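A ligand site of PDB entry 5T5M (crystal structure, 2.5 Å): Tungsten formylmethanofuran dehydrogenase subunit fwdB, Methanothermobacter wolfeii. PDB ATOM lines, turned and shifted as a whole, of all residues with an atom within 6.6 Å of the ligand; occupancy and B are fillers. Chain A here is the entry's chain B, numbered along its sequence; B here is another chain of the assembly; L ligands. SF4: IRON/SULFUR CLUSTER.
The backbone NH (N) of Cys 35 lies close to a sulfur (S2) of the ligand, 3.8 Å away.
The side-chain sulfur (SG) of Cys 35 is bound to an iron atom (FE3) of the ligand, 2.4 Å away.
FE4 of the ligand is bound by SG of Cys 9 (2.4 Å).
The backbone NH (N) of Cys 16 sits close to a sulfur (S3) of the ligand (3.8 Å).
The side-chain sulfur (SG) of Cys 16 is bound to an iron atom (FE1) of the ligand (2.5 Å).
The side-chain sulfur of Cys 12 binds an iron atom (FE2) of the ligand, 2.5 Å away.
The side-chain sulfur of Cys 35 lies close to the backbone NH of Gly 38.
The backbone NH (N) of Ile 37 lies close to the side-chain sulfur (SG) of Cys 35 (3.6 Å).
The backbone carbonyl oxygen (O) of Cys 16 sits at hydrogen-bond distance from the backbone NH (N) of Cys 9, at 2.8 Å.
The side-chain sulfur (SG) of Cys 9 lies close to the backbone NH (N) of Phe 11 (3.6 Å).
The side-chain sulfur of Cys 16 lies close to the guanidinium group of Arg 159, at 3.2 Å.
N of Thr 14 of chain A lies close to SG of Cys 12, at 3.1 Å.
The guanidinium group (NE) of Arg 159 lies within hydrogen-bond range of the backbone carbonyl oxygen (O) of Asn 33 (3.0 Å).
O of Thr 14 of chain A is in hydrogen-bond range of NH1 of Arg 163, 3.1 Å away.
Residues that only touch the ligand: Gly 38, Leu 15, Arg 159, Thr 14 of chain A and Phe 11.
Within 4 Å of the ligand: Cys 9, Phe 11, Cys 12, Thr 14 of chain A, Leu 15, Cys 16, Cys 35, Gly 38 and Arg 159.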
ATOM      1  N   CYS A   9      14.224  25.131 -30.683  1.00  0.00           N
ATOM      2  CA  CYS A   9      13.655  26.294 -30.012  1.00  0.00           C
ATOM      3  C   CYS A   9      14.725  27.024 -29.200  1.00  0.00           C
ATOM      4  O   CYS A   9      15.410  26.393 -28.374  1.00  0.00           O
ATOM      5  CB  CYS A   9      12.536  25.893 -29.064  1.00  0.00           C
ATOM      6  SG  CYS A   9      12.023  27.300 -28.110  1.00  0.00           S
ATOM      7  N   PRO A  10      14.881  28.360 -29.374  1.00  0.00           N
ATOM      8  CA  PRO A  10      15.868  29.093 -28.574  1.00  0.00           C
ATOM      9  C   PRO A  10      15.268  29.777 -27.354  1.00  0.00           C
ATOM     10  O   PRO A  10      15.337  31.001 -27.240  1.00  0.00           O
ATOM     11  CB  PRO A  10      16.404  30.125 -29.571  1.00  0.00           C
ATOM     12  CG  PRO A  10      15.179  30.467 -30.366  1.00  0.00           C
ATOM     13  CD  PRO A  10      14.371  29.190 -30.476  1.00  0.00           C
ATOM     14  N   PHE A  11      14.664  29.005 -26.448  1.00  0.00           N
ATOM     15  CA  PHE A  11      14.299  29.613 -25.166  1.00  0.00           C
ATOM     16  C   PHE A  11      14.887  28.866 -23.971  1.00  0.00           C
ATOM     17  O   PHE A  11      15.869  29.340 -23.387  1.00  0.00           O
ATOM     18  CB  PHE A  11      12.793  29.689 -24.994  1.00  0.00           C
ATOM     19  CG  PHE A  11      12.409  30.375 -23.722  1.00  0.00           C
ATOM     20  CD1 PHE A  11      12.472  31.757 -23.627  1.00  0.00           C
ATOM     21  CD2 PHE A  11      12.038  29.647 -22.620  1.00  0.00           C
ATOM     22  CE1 PHE A  11      12.139  32.400 -22.463  1.00  0.00           C
ATOM     23  CE2 PHE A  11      11.708  30.279 -21.443  1.00  0.00           C
ATOM     24  CZ  PHE A  11      11.752  31.656 -21.362  1.00  0.00           C
ATOM     25  N   CYS A  12      14.307  27.738 -23.593  1.00  0.00           N
ATOM     26  CA  CYS A  12      14.685  27.071 -22.359  1.00  0.00           C
ATOM     27  C   CYS A  12      15.592  25.876 -22.640  1.00  0.00           C
ATOM     28  O   CYS A  12      15.778  25.442 -23.782  1.00  0.00           O
ATOM     29  CB  CYS A  12      13.429  26.649 -21.585  1.00  0.00           C
ATOM     30  SG  CYS A  12      13.048  24.940 -21.629  1.00  0.00           S
ATOM     31  N   GLY A  13      16.170  25.345 -21.559  1.00  0.00           N
ATOM     32  CA  GLY A  13      17.147  24.276 -21.640  1.00  0.00           C
ATOM     33  C   GLY A  13      16.593  22.911 -22.036  1.00  0.00           C
ATOM     34  O   GLY A  13      17.368  21.963 -22.181  1.00  0.00           O
ATOM     35  N   THR A  14      15.283  22.798 -22.210  1.00  0.00           N
ATOM     36  CA  THR A  14      14.731  21.584 -22.800  1.00  0.00           C
ATOM     37  C   THR A  14      15.187  21.422 -24.245  1.00  0.00           C
ATOM     38  O   THR A  14      15.355  20.295 -24.714  1.00  0.00           O
ATOM     39  CB  THR A  14      13.209  21.625 -22.688  1.00  0.00           C
ATOM     40  OG1 THR A  14      12.833  21.788 -21.308  1.00  0.00           O
ATOM     41  CG2 THR A  14      12.619  20.338 -23.232  1.00  0.00           C
ATOM     42  N   LEU A  15      15.392  22.538 -24.944  1.00  0.00           N
ATOM     43  CA  LEU A  15      15.950  22.577 -26.299  1.00  0.00           C
ATOM     44  C   LEU A  15      15.202  21.643 -27.257  1.00  0.00           C
ATOM     45  O   LEU A  15      15.774  20.774 -27.918  1.00  0.00           O
ATOM     46  CB  LEU A  15      17.446  22.247 -26.274  1.00  0.00           C
ATOM     47  CG  LEU A  15      18.257  22.850 -27.416  1.00  0.00           C
ATOM     48  CD1 LEU A  15      18.241  24.362 -27.355  1.00  0.00           C
ATOM     49  CD2 LEU A  15      19.698  22.343 -27.383  1.00  0.00           C
ATOM     50  N   CYS A  16      13.893  21.869 -27.350  1.00  0.00           N
ATOM     51  CA  CYS A  16      13.074  21.080 -28.251  1.00  0.00           C
ATOM     52  C   CYS A  16      13.538  21.299 -29.695  1.00  0.00           C
ATOM     53  O   CYS A  16      13.688  22.440 -30.139  1.00  0.00           O
ATOM     54  CB  CYS A  16      11.608  21.454 -28.103  1.00  0.00           C
ATOM     55  SG  CYS A  16      10.921  20.968 -26.500  1.00  0.00           S
ATOM     56  N   ASP A  17      13.776  20.205 -30.401  1.00  0.00           N
ATOM     57  CA  ASP A  17      14.236  20.246 -31.773  1.00  0.00           C
ATOM     58  C   ASP A  17      13.187  19.730 -32.750  1.00  0.00           C
ATOM     59  O   ASP A  17      13.514  19.240 -33.833  1.00  0.00           O
ATOM     60  CB  ASP A  17      15.532  19.447 -31.919  1.00  0.00           C
ATOM     61  CG  ASP A  17      15.335  17.966 -31.686  1.00  0.00           C
ATOM     62  OD1 ASP A  17      14.487  17.592 -30.839  1.00  0.00           O
ATOM     63  OD2 ASP A  17      16.015  17.169 -32.378  1.00  0.00           O
ATOM     64  N   ASP A  18      11.904  19.840 -32.387  1.00  0.00           N
ATOM     65  CA  ASP A  18      10.793  19.388 -33.216  1.00  0.00           C
ATOM     66  C   ASP A  18       9.821  20.526 -33.508  1.00  0.00           C
ATOM     67  O   ASP A  18       8.638  20.292 -33.751  1.00  0.00           O
ATOM     68  CB  ASP A  18      10.054  18.230 -32.548  1.00  0.00           C
ATOM     69  CG  ASP A  18       9.475  18.640 -31.208  1.00  0.00           C
ATOM     70  OD1 ASP A  18       9.948  19.663 -30.676  1.00  0.00           O
ATOM     71  OD2 ASP A  18       8.551  17.957 -30.705  1.00  0.00           O
ATOM     72  N   ILE A  19      10.302  21.762 -33.472  1.00  0.00           N
ATOM     73  CA  ILE A  19       9.422  22.909 -33.715  1.00  0.00           C
ATOM     74  C   ILE A  19       9.173  23.026 -35.211  1.00  0.00           C
ATOM     75  O   ILE A  19      10.052  22.766 -36.037  1.00  0.00           O
ATOM     76  CB  ILE A  19      10.026  24.198 -33.143  1.00  0.00           C
ATOM     77  CG1 ILE A  19      10.399  24.032 -31.663  1.00  0.00           C
ATOM     78  CG2 ILE A  19       9.064  25.355 -33.334  1.00  0.00           C
ATOM     79  CD1 ILE A  19       9.256  23.589 -30.770  1.00  0.00           C
ATOM     80  N   ASN A  33       3.834  22.809 -32.233  1.00  0.00           N
ATOM     81  CA  ASN A  33       4.523  22.006 -31.209  1.00  0.00           C
ATOM     82  C   ASN A  33       5.186  22.856 -30.124  1.00  0.00           C
ATOM     83  O   ASN A  33       5.306  22.407 -28.973  1.00  0.00           O
ATOM     84  CB  ASN A  33       5.552  21.061 -31.856  1.00  0.00           C
ATOM     85  CG  ASN A  33       4.883  19.912 -32.654  1.00  0.00           C
ATOM     86  OD1 ASN A  33       3.741  19.537 -32.404  1.00  0.00           O
ATOM     87  ND2 ASN A  33       5.624  19.346 -33.592  1.00  0.00           N
ATOM     88  N   ALA A  34       5.597  24.076 -30.446  1.00  0.00           N
ATOM     89  CA  ALA A  34       6.206  24.965 -29.447  1.00  0.00           C
ATOM     90  C   ALA A  34       5.211  25.278 -28.326  1.00  0.00           C
ATOM     91  O   ALA A  34       4.016  25.420 -28.561  1.00  0.00           O
ATOM     92  CB  ALA A  34       6.665  26.258 -30.110  1.00  0.00           C
ATOM     93  N   CYS A  35       5.735  25.399 -27.101  1.00  0.00           N
ATOM     94  CA  CYS A  35       4.899  25.781 -25.979  1.00  0.00           C
ATOM     95  C   CYS A  35       4.627  27.290 -26.013  1.00  0.00           C
ATOM     96  O   CYS A  35       5.186  28.028 -26.819  1.00  0.00           O
ATOM     97  CB  CYS A  35       5.544  25.363 -24.649  1.00  0.00           C
ATOM     98  SG  CYS A  35       6.890  26.388 -24.094  1.00  0.00           S
ATOM     99  N   ARG A  36       3.743  27.744 -25.119  1.00  0.00           N
ATOM    100  CA  ARG A  36       3.325  29.144 -25.122  1.00  0.00           C
ATOM    101  C   ARG A  36       4.525  30.086 -25.034  1.00  0.00           C
ATOM    102  O   ARG A  36       4.496  31.169 -25.629  1.00  0.00           O
ATOM    103  CB  ARG A  36       2.352  29.409 -23.989  1.00  0.00           C
ATOM    104  CG  ARG A  36       1.963  30.879 -23.827  1.00  0.00           C
ATOM    105  CD  ARG A  36       1.170  31.106 -22.566  1.00  0.00           C
ATOM    106  NE  ARG A  36      -0.202  30.595 -22.656  1.00  0.00           N
ATOM    107  CZ  ARG A  36      -1.203  31.252 -23.224  1.00  0.00           C
ATOM    108  NH1 ARG A  36      -1.008  32.441 -23.772  1.00  0.00           N
ATOM    109  NH2 ARG A  36      -2.413  30.721 -23.241  1.00  0.00           N
ATOM    110  N   ILE A  37       5.567  29.719 -24.292  1.00  0.00           N
ATOM    111  CA  ILE A  37       6.762  30.571 -24.227  1.00  0.00           C
ATOM    112  C   ILE A  37       7.518  30.512 -25.545  1.00  0.00           C
ATOM    113  O   ILE A  37       7.790  31.532 -26.176  1.00  0.00           O
ATOM    114  CB  ILE A  37       7.670  30.181 -23.061  1.00  0.00           C
ATOM    115  CG1 ILE A  37       6.879  30.070 -21.742  1.00  0.00           C
ATOM    116  CG2 ILE A  37       8.774  31.218 -22.915  1.00  0.00           C
ATOM    117  CD1 ILE A  37       7.702  29.543 -20.584  1.00  0.00           C
ATOM    118  N   GLY A  38       7.897  29.302 -25.955  1.00  0.00           N
ATOM    119  CA  GLY A  38       8.608  29.135 -27.215  1.00  0.00           C
ATOM    120  C   GLY A  38       7.942  29.880 -28.367  1.00  0.00           C
ATOM    121  O   GLY A  38       8.606  30.570 -29.142  1.00  0.00           O
ATOM    122  N   HIS A  39       6.614  29.741 -28.484  1.00  0.00           N
ATOM    123  CA  HIS A  39       5.901  30.466 -29.520  1.00  0.00           C
ATOM    124  C   HIS A  39       6.129  31.965 -29.409  1.00  0.00           C
ATOM    125  O   HIS A  39       6.226  32.660 -30.429  1.00  0.00           O
ATOM    126  CB  HIS A  39       4.411  30.147 -29.437  1.00  0.00           C
ATOM    127  CG  HIS A  39       3.561  30.958 -30.368  1.00  0.00           C
ATOM    128  ND1 HIS A  39       3.523  30.734 -31.728  1.00  0.00           N
ATOM    129  CD2 HIS A  39       2.719  31.989 -30.135  1.00  0.00           C
ATOM    130  CE1 HIS A  39       2.678  31.596 -32.286  1.00  0.00           C
ATOM    131  NE2 HIS A  39       2.180  32.367 -31.339  1.00  0.00           N
ATOM    132  N   PHE A  42       9.524  33.009 -31.015  1.00  0.00           N
ATOM    133  CA  PHE A  42       9.521  32.879 -32.471  1.00  0.00           C
ATOM    134  C   PHE A  42       8.732  33.992 -33.149  1.00  0.00           C
ATOM    135  O   PHE A  42       9.037  34.348 -34.294  1.00  0.00           O
ATOM    136  CB  PHE A  42       8.941  31.530 -32.888  1.00  0.00           C
ATOM    137  CG  PHE A  42       9.916  30.403 -32.807  1.00  0.00           C
ATOM    138  CD1 PHE A  42      11.012  30.364 -33.645  1.00  0.00           C
ATOM    139  CD2 PHE A  42       9.735  29.385 -31.885  1.00  0.00           C
ATOM    140  CE1 PHE A  42      11.914  29.334 -33.567  1.00  0.00           C
ATOM    141  CE2 PHE A  42      10.636  28.341 -31.803  1.00  0.00           C
ATOM    142  CZ  PHE A  42      11.726  28.309 -32.641  1.00  0.00           C
ATOM    143  N   ALA A 156       8.217  26.643 -16.311  1.00  0.00           N
ATOM    144  CA  ALA A 156       9.555  27.037 -16.727  1.00  0.00           C
ATOM    145  C   ALA A 156      10.182  26.092 -17.747  1.00  0.00           C
ATOM    146  O   ALA A 156      11.157  26.479 -18.403  1.00  0.00           O
ATOM    147  CB  ALA A 156      10.470  27.144 -15.502  1.00  0.00           C
ATOM    148  N   HIS A 157       9.711  24.870 -17.898  1.00  0.00           N
ATOM    149  CA  HIS A 157      10.159  23.973 -18.953  1.00  0.00           C
ATOM    150  C   HIS A 157       8.918  23.247 -19.439  1.00  0.00           C
ATOM    151  O   HIS A 157       8.730  22.053 -19.174  1.00  0.00           O
ATOM    152  CB  HIS A 157      11.228  23.000 -18.460  1.00  0.00           C
ATOM    153  CG  HIS A 157      12.474  23.651 -17.928  1.00  0.00           C
ATOM    154  ND1 HIS A 157      12.581  24.088 -16.625  1.00  0.00           N
ATOM    155  CD2 HIS A 157      13.674  23.900 -18.509  1.00  0.00           C
ATOM    156  CE1 HIS A 157      13.786  24.588 -16.433  1.00  0.00           C
ATOM    157  NE2 HIS A 157      14.468  24.490 -17.556  1.00  0.00           N
ATOM    158  N   PRO A 158       8.012  23.958 -20.115  1.00  0.00           N
ATOM    159  CA  PRO A 158       6.636  23.454 -20.228  1.00  0.00           C
ATOM    160  C   PRO A 158       6.510  22.088 -20.877  1.00  0.00           C
ATOM    161  O   PRO A 158       5.663  21.291 -20.443  1.00  0.00           O
ATOM    162  CB  PRO A 158       5.936  24.558 -21.024  1.00  0.00           C
ATOM    163  CG  PRO A 158       6.719  25.821 -20.643  1.00  0.00           C
ATOM    164  CD  PRO A 158       8.139  25.336 -20.611  1.00  0.00           C
ATOM    165  N   ARG A 159       7.327  21.754 -21.880  1.00  0.00           N
ATOM    166  CA  ARG A 159       7.194  20.462 -22.553  1.00  0.00           C
ATOM    167  C   ARG A 159       8.080  19.395 -21.937  1.00  0.00           C
ATOM    168  O   ARG A 159       8.153  18.283 -22.474  1.00  0.00           O
ATOM    169  CB  ARG A 159       7.496  20.606 -24.038  1.00  0.00           C
ATOM    170  CG  ARG A 159       6.594  21.594 -24.754  1.00  0.00           C
ATOM    171  CD  ARG A 159       7.000  21.743 -26.204  1.00  0.00           C
ATOM    172  NE  ARG A 159       6.570  20.599 -27.011  1.00  0.00           N
ATOM    173  CZ  ARG A 159       7.234  20.130 -28.059  1.00  0.00           C
ATOM    174  NH1 ARG A 159       8.380  20.689 -28.448  1.00  0.00           N
ATOM    175  NH2 ARG A 159       6.764  19.098 -28.731  1.00  0.00           N
ATOM    176  N   HIS A 160       8.745  19.696 -20.821  1.00  0.00           N
ATOM    177  CA  HIS A 160       9.680  18.757 -20.227  1.00  0.00           C
ATOM    178  C   HIS A 160       8.984  17.487 -19.739  1.00  0.00           C
ATOM    179  O   HIS A 160       9.464  16.374 -19.969  1.00  0.00           O
ATOM    180  CB  HIS A 160      10.423  19.453 -19.090  1.00  0.00           C
ATOM    181  CG  HIS A 160      11.670  18.754 -18.671  1.00  0.00           C
ATOM    182  ND1 HIS A 160      11.673  17.714 -17.768  1.00  0.00           N
ATOM    183  CD2 HIS A 160      12.975  18.956 -19.014  1.00  0.00           C
ATOM    184  CE1 HIS A 160      12.920  17.301 -17.563  1.00  0.00           C
ATOM    185  NE2 HIS A 160      13.725  18.043 -18.316  1.00  0.00           N
ATOM    186  N   ARG A 163       7.657  15.374 -22.649  1.00  0.00           N
ATOM    187  CA  ARG A 163       8.749  14.732 -23.371  1.00  0.00           C
ATOM    188  C   ARG A 163       9.425  13.634 -22.559  1.00  0.00           C
ATOM    189  O   ARG A 163       9.936  12.672 -23.141  1.00  0.00           O
ATOM    190  CB  ARG A 163       9.764  15.783 -23.826  1.00  0.00           C
ATOM    191  CG  ARG A 163       9.288  16.651 -25.015  1.00  0.00           C
ATOM    192  CD  ARG A 163      10.417  17.557 -25.526  1.00  0.00           C
ATOM    193  NE  ARG A 163      11.617  16.803 -25.847  1.00  0.00           N
ATOM    194  CZ  ARG A 163      12.829  17.335 -26.006  1.00  0.00           C
ATOM    195  NH1 ARG A 163      13.016  18.631 -25.881  1.00  0.00           N
ATOM    196  NH2 ARG A 163      13.860  16.548 -26.293  1.00  0.00           N
ATOM    197  N   TYR A 291      18.348  28.149 -23.178  1.00  0.00           N
ATOM    198  CA  TYR A 291      18.600  27.087 -24.147  1.00  0.00           C
ATOM    199  C   TYR A 291      20.086  26.875 -24.388  1.00  0.00           C
ATOM    200  O   TYR A 291      20.475  25.771 -24.792  1.00  0.00           O
ATOM    201  CB  TYR A 291      17.883  27.396 -25.466  1.00  0.00           C
ATOM    202  CG  TYR A 291      18.529  28.478 -26.291  1.00  0.00           C
ATOM    203  CD1 TYR A 291      18.233  29.820 -26.067  1.00  0.00           C
ATOM    204  CD2 TYR A 291      19.405  28.170 -27.329  1.00  0.00           C
ATOM    205  CE1 TYR A 291      18.808  30.828 -26.827  1.00  0.00           C
ATOM    206  CE2 TYR A 291      19.980  29.164 -28.085  1.00  0.00           C
ATOM    207  CZ  TYR A 291      19.682  30.492 -27.834  1.00  0.00           C
ATOM    208  OH  TYR A 291      20.252  31.480 -28.608  1.00  0.00           O
ATOM    209  N   GLY B  14       0.444  25.134 -23.468  1.00  0.00           N
ATOM    210  CA  GLY B  14       1.026  24.495 -24.623  1.00  0.00           C
ATOM    211  C   GLY B  14       2.046  23.453 -24.224  1.00  0.00           C
ATOM    212  O   GLY B  14       2.982  23.185 -24.987  1.00  0.00           O
HETATM  213 FE1  SF4 L   1      10.658  23.290 -25.711  1.00  0.00          FE
HETATM  214 FE2  SF4 L   1      11.499  25.286 -23.590  1.00  0.00          FE
HETATM  215 FE3  SF4 L   1       8.853  25.182 -24.615  1.00  0.00          FE
HETATM  216 FE4  SF4 L   1      10.939  26.081 -26.287  1.00  0.00          FE
HETATM  217  S1  SF4 L   1      10.189  26.661 -24.460  1.00  0.00           S
HETATM  218  S2  SF4 L   1       9.433  24.812 -26.456  1.00  0.00           S
HETATM  219  S3  SF4 L   1      12.140  24.600 -25.440  1.00  0.00           S
HETATM  220  S4  SF4 L   1      10.131  23.826 -23.819  1.00  0.00           S
